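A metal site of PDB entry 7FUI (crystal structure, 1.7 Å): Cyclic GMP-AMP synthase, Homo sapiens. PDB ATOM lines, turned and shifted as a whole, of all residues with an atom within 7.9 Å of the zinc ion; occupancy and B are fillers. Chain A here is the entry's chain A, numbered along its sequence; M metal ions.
Of the 18 residues printed, 4 come within 4 Å of the zinc ion. The nearest printed residue that does not touch the zinc ion is Arg 246 (4.2 Å).
NE of Arg 246 is in hydrogen-bond range of O of His 230 (3.4 Å). ND1 of His 230 is in hydrogen-bond range of O of Leu 227, 3.1 Å away. The backbone NH of Cys 237 is in hydrogen-bond range of the backbone carbonyl oxygen of Glu 242 (2.8 Å). The guanidinium group (NH2) of Arg 246 lies close to the side-chain sulfur (SG) of Cys 236 (3.6 Å). The guanidinium group (NH2) of Arg 246 lies close to the side-chain sulfur (SG) of Cys 244 (3.5 Å). O of Cys 237 is in hydrogen-bond range of NZ of Lys 243, at 3.4 Å.
The zinc ion is bound by NE2 of His 230 (2.1 Å), SG of Cys 237 (2.2 Å), SG of Cys 236 (2.3 Å) and SG of Cys 244 (2.4 Å).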
ATOM      1  N   LEU A 227      20.676 -31.307  10.978  1.00  0.00           N
ATOM      2  CA  LEU A 227      21.917 -31.701  10.278  1.00  0.00           C
ATOM      3  C   LEU A 227      22.647 -30.494   9.703  1.00  0.00           C
ATOM      4  O   LEU A 227      23.883 -30.549   9.637  1.00  0.00           O
ATOM      5  CB  LEU A 227      21.595 -32.768   9.231  1.00  0.00           C
ATOM      6  CG  LEU A 227      21.546 -34.168   9.811  1.00  0.00           C
ATOM      7  CD1 LEU A 227      21.037 -35.172   8.797  1.00  0.00           C
ATOM      8  CD2 LEU A 227      22.934 -34.572  10.351  1.00  0.00           C
ATOM      9  N   ASN A 229      22.552 -27.484  10.996  1.00  0.00           N
ATOM     10  CA  ASN A 229      22.843 -26.543  12.112  1.00  0.00           C
ATOM     11  C   ASN A 229      23.092 -27.391  13.345  1.00  0.00           C
ATOM     12  O   ASN A 229      22.308 -27.371  14.286  1.00  0.00           O
ATOM     13  CB  ASN A 229      21.753 -25.490  12.222  1.00  0.00           C
ATOM     14  CG  ASN A 229      22.207 -24.278  13.018  1.00  0.00           C
ATOM     15  OD1 ASN A 229      23.343 -24.232  13.529  1.00  0.00           O
ATOM     16  ND2 ASN A 229      21.339 -23.298  13.093  1.00  0.00           N
ATOM     17  N   HIS A 230      24.228 -28.095  13.319  1.00  0.00           N
ATOM     18  CA  HIS A 230      24.431 -29.370  14.022  1.00  0.00           C
ATOM     19  C   HIS A 230      25.417 -29.254  15.193  1.00  0.00           C
ATOM     20  O   HIS A 230      25.655 -30.281  15.805  1.00  0.00           O
ATOM     21  CB  HIS A 230      24.915 -30.428  13.006  1.00  0.00           C
ATOM     22  CG  HIS A 230      26.268 -30.106  12.489  1.00  0.00           C
ATOM     23  ND1 HIS A 230      26.513 -29.883  11.168  1.00  0.00           N
ATOM     24  CD2 HIS A 230      27.443 -29.881  13.135  1.00  0.00           C
ATOM     25  CE1 HIS A 230      27.777 -29.556  11.016  1.00  0.00           C
ATOM     26  NE2 HIS A 230      28.366 -29.579  12.202  1.00  0.00           N
ATOM     27  N   GLY A 231      26.019 -28.091  15.470  1.00  0.00           N
ATOM     28  CA  GLY A 231      27.024 -27.970  16.544  1.00  0.00           C
ATOM     29  C   GLY A 231      26.467 -27.300  17.791  1.00  0.00           C
ATOM     30  O   GLY A 231      25.415 -26.610  17.697  1.00  0.00           O
ATOM     31  N   LYS A 232      27.123 -27.475  18.937  1.00  0.00           N
ATOM     32  CA  LYS A 232      26.846 -26.654  20.136  1.00  0.00           C
ATOM     33  C   LYS A 232      27.277 -25.210  19.813  1.00  0.00           C
ATOM     34  O   LYS A 232      26.543 -24.245  20.173  1.00  0.00           O
ATOM     35  CB  LYS A 232      27.607 -27.151  21.359  1.00  0.00           C
ATOM     36  CG  LYS A 232      27.397 -26.270  22.587  1.00  0.00           C
ATOM     37  CD  LYS A 232      27.888 -26.874  23.882  1.00  0.00           C
ATOM     38  CE  LYS A 232      27.016 -27.988  24.415  1.00  0.00           C
ATOM     39  NZ  LYS A 232      25.597 -27.609  24.532  1.00  0.00           N
ATOM     40  N   SER A 233      28.444 -25.054  19.184  1.00  0.00           N
ATOM     41  CA  SER A 233      28.932 -23.752  18.650  1.00  0.00           C
ATOM     42  C   SER A 233      28.115 -23.392  17.408  1.00  0.00           C
ATOM     43  O   SER A 233      27.958 -24.238  16.536  1.00  0.00           O
ATOM     44  CB  SER A 233      30.378 -23.763  18.337  1.00  0.00           C
ATOM     45  OG  SER A 233      30.713 -22.607  17.594  1.00  0.00           O
ATOM     46  N   THR A 235      29.137 -21.521  15.135  1.00  0.00           N
ATOM     47  CA  THR A 235      30.118 -21.462  14.031  1.00  0.00           C
ATOM     48  C   THR A 235      30.691 -22.864  13.788  1.00  0.00           C
ATOM     49  O   THR A 235      31.761 -22.922  13.162  1.00  0.00           O
ATOM     50  CB  THR A 235      31.179 -20.384  14.302  1.00  0.00           C
ATOM     51  OG1 THR A 235      31.723 -20.528  15.607  1.00  0.00           O
ATOM     52  CG2 THR A 235      30.586 -18.998  14.206  1.00  0.00           C
ATOM     53  N   CYS A 236      30.073 -23.942  14.294  1.00  0.00           N
ATOM     54  CA  CYS A 236      30.540 -25.324  14.019  1.00  0.00           C
ATOM     55  C   CYS A 236      30.634 -25.474  12.496  1.00  0.00           C
ATOM     56  O   CYS A 236      29.672 -25.134  11.799  1.00  0.00           O
ATOM     57  CB  CYS A 236      29.697 -26.413  14.661  1.00  0.00           C
ATOM     58  SG  CYS A 236      30.493 -28.055  14.655  1.00  0.00           S
ATOM     59  N   CYS A 237      31.802 -25.873  11.997  1.00  0.00           N
ATOM     60  CA  CYS A 237      32.064 -26.190  10.566  1.00  0.00           C
ATOM     61  C   CYS A 237      31.990 -24.942   9.652  1.00  0.00           C
ATOM     62  O   CYS A 237      31.836 -25.102   8.417  1.00  0.00           O
ATOM     63  CB  CYS A 237      31.082 -27.249  10.068  1.00  0.00           C
ATOM     64  SG  CYS A 237      31.452 -28.878  10.760  1.00  0.00           S
ATOM     65  N   GLU A 238      32.079 -23.723  10.202  1.00  0.00           N
ATOM     66  CA  GLU A 238      32.148 -22.480   9.388  1.00  0.00           C
ATOM     67  C   GLU A 238      33.608 -22.022   9.250  1.00  0.00           C
ATOM     68  O   GLU A 238      33.858 -21.133   8.443  1.00  0.00           O
ATOM     69  CB  GLU A 238      31.296 -21.354   9.995  1.00  0.00           C
ATOM     70  CG  GLU A 238      29.804 -21.581   9.857  1.00  0.00           C
ATOM     71  CD  GLU A 238      28.941 -20.363  10.134  1.00  0.00           C
ATOM     72  OE1 GLU A 238      29.465 -19.341  10.627  1.00  0.00           O
ATOM     73  OE2 GLU A 238      27.771 -20.424   9.787  1.00  0.00           O
ATOM     74  N   GLU A 242      37.017 -25.274  13.569  1.00  0.00           N
ATOM     75  CA  GLU A 242      35.761 -25.832  14.150  1.00  0.00           C
ATOM     76  C   GLU A 242      35.170 -26.917  13.233  1.00  0.00           C
ATOM     77  O   GLU A 242      33.955 -27.147  13.313  1.00  0.00           O
ATOM     78  CB  GLU A 242      34.743 -24.709  14.393  1.00  0.00           C
ATOM     79  CG  GLU A 242      35.023 -23.914  15.664  1.00  0.00           C
ATOM     80  CD  GLU A 242      33.886 -23.001  16.085  1.00  0.00           C
ATOM     81  OE1 GLU A 242      33.005 -23.458  16.829  1.00  0.00           O
ATOM     82  OE2 GLU A 242      33.878 -21.843  15.641  1.00  0.00           O
ATOM     83  N   LYS A 243      36.004 -27.610  12.454  1.00  0.00           N
ATOM     84  CA  LYS A 243      35.528 -28.639  11.475  1.00  0.00           C
ATOM     85  C   LYS A 243      35.293 -29.929  12.255  1.00  0.00           C
ATOM     86  O   LYS A 243      36.290 -30.600  12.549  1.00  0.00           O
ATOM     87  CB  LYS A 243      36.542 -28.846  10.348  1.00  0.00           C
ATOM     88  CG  LYS A 243      36.693 -27.662   9.397  1.00  0.00           C
ATOM     89  CD  LYS A 243      35.485 -27.408   8.519  1.00  0.00           C
ATOM     90  CE  LYS A 243      35.709 -26.308   7.505  1.00  0.00           C
ATOM     91  NZ  LYS A 243      34.530 -26.092   6.643  1.00  0.00           N
ATOM     92  N   CYS A 244      34.057 -30.252  12.616  1.00  0.00           N
ATOM     93  CA  CYS A 244      33.769 -31.493  13.389  1.00  0.00           C
ATOM     94  C   CYS A 244      33.644 -32.656  12.408  1.00  0.00           C
ATOM     95  O   CYS A 244      33.656 -32.429  11.180  1.00  0.00           O
ATOM     96  CB  CYS A 244      32.554 -31.322  14.290  1.00  0.00           C
ATOM     97  SG  CYS A 244      30.966 -31.418  13.434  1.00  0.00           S
ATOM     98  N   CYS A 245      33.517 -33.874  12.908  1.00  0.00           N
ATOM     99  CA  CYS A 245      33.396 -35.086  12.052  1.00  0.00           C
ATOM    100  C   CYS A 245      31.996 -35.700  12.161  1.00  0.00           C
ATOM    101  O   CYS A 245      31.806 -36.877  11.690  1.00  0.00           O
ATOM    102  CB  CYS A 245      34.489 -36.093  12.389  1.00  0.00           C
ATOM    103  SG  CYS A 245      34.327 -36.824  14.032  1.00  0.00           S
ATOM    104  N   ARG A 246      30.990 -34.944  12.619  1.00  0.00           N
ATOM    105  CA  ARG A 246      29.613 -35.460  12.770  1.00  0.00           C
ATOM    106  C   ARG A 246      29.094 -35.993  11.432  1.00  0.00           C
ATOM    107  O   ARG A 246      28.701 -37.177  11.383  1.00  0.00           O
ATOM    108  CB  ARG A 246      28.632 -34.414  13.303  1.00  0.00           C
ATOM    109  CG  ARG A 246      28.705 -34.260  14.818  1.00  0.00           C
ATOM    110  CD  ARG A 246      27.745 -33.163  15.225  1.00  0.00           C
ATOM    111  NE  ARG A 246      27.779 -32.813  16.636  1.00  0.00           N
ATOM    112  CZ  ARG A 246      28.446 -31.775  17.129  1.00  0.00           C
ATOM    113  NH1 ARG A 246      28.328 -31.477  18.412  1.00  0.00           N
ATOM    114  NH2 ARG A 246      29.149 -30.985  16.342  1.00  0.00           N
ATOM    115  N   LYS A 247      29.118 -35.175  10.390  1.00  0.00           N
ATOM    116  CA  LYS A 247      28.572 -35.605   9.083  1.00  0.00           C
ATOM    117  C   LYS A 247      29.444 -36.726   8.483  1.00  0.00           C
ATOM    118  O   LYS A 247      28.871 -37.585   7.825  1.00  0.00           O
ATOM    119  CB  LYS A 247      28.407 -34.406   8.147  1.00  0.00           C
ATOM    120  CG  LYS A 247      27.295 -33.449   8.563  1.00  0.00           C
ATOM    121  CD  LYS A 247      26.886 -32.520   7.448  1.00  0.00           C
ATOM    122  CE  LYS A 247      25.596 -31.791   7.731  1.00  0.00           C
ATOM    123  NZ  LYS A 247      25.326 -30.796   6.688  1.00  0.00           N
ATOM    124  N   ASP A 292      30.975 -30.258  20.888  1.00  0.00           N
ATOM    125  CA  ASP A 292      31.728 -30.300  19.605  1.00  0.00           C
ATOM    126  C   ASP A 292      33.093 -30.982  19.788  1.00  0.00           C
ATOM    127  O   ASP A 292      33.591 -31.594  18.806  1.00  0.00           O
ATOM    128  CB  ASP A 292      31.885 -28.902  19.039  1.00  0.00           C
ATOM    129  CG  ASP A 292      30.537 -28.250  18.747  1.00  0.00           C
ATOM    130  OD1 ASP A 292      29.553 -28.991  18.649  1.00  0.00           O
ATOM    131  OD2 ASP A 292      30.491 -26.994  18.631  1.00  0.00           O
ATOM    132  N   TRP A 295      33.594 -34.555  18.880  1.00  0.00           N
ATOM    133  CA  TRP A 295      33.508 -34.759  17.412  1.00  0.00           C
ATOM    134  C   TRP A 295      34.679 -34.059  16.705  1.00  0.00           C
ATOM    135  O   TRP A 295      34.550 -33.669  15.550  1.00  0.00           O
ATOM    136  CB  TRP A 295      32.148 -34.272  16.854  1.00  0.00           C
ATOM    137  CG  TRP A 295      30.998 -35.005  17.443  1.00  0.00           C
ATOM    138  CD1 TRP A 295      30.235 -34.608  18.505  1.00  0.00           C
ATOM    139  CD2 TRP A 295      30.447 -36.266  17.006  1.00  0.00           C
ATOM    140  NE1 TRP A 295      29.260 -35.530  18.770  1.00  0.00           N
ATOM    141  CE2 TRP A 295      29.364 -36.571  17.868  1.00  0.00           C
ATOM    142  CE3 TRP A 295      30.729 -37.131  15.954  1.00  0.00           C
ATOM    143  CZ2 TRP A 295      28.601 -37.724  17.724  1.00  0.00           C
ATOM    144  CZ3 TRP A 295      29.991 -38.290  15.823  1.00  0.00           C
ATOM    145  CH2 TRP A 295      28.935 -38.572  16.689  1.00  0.00           C
HETATM  146 ZN    ZN M   1      30.351 -29.279  12.659  1.00  0.00          ZN
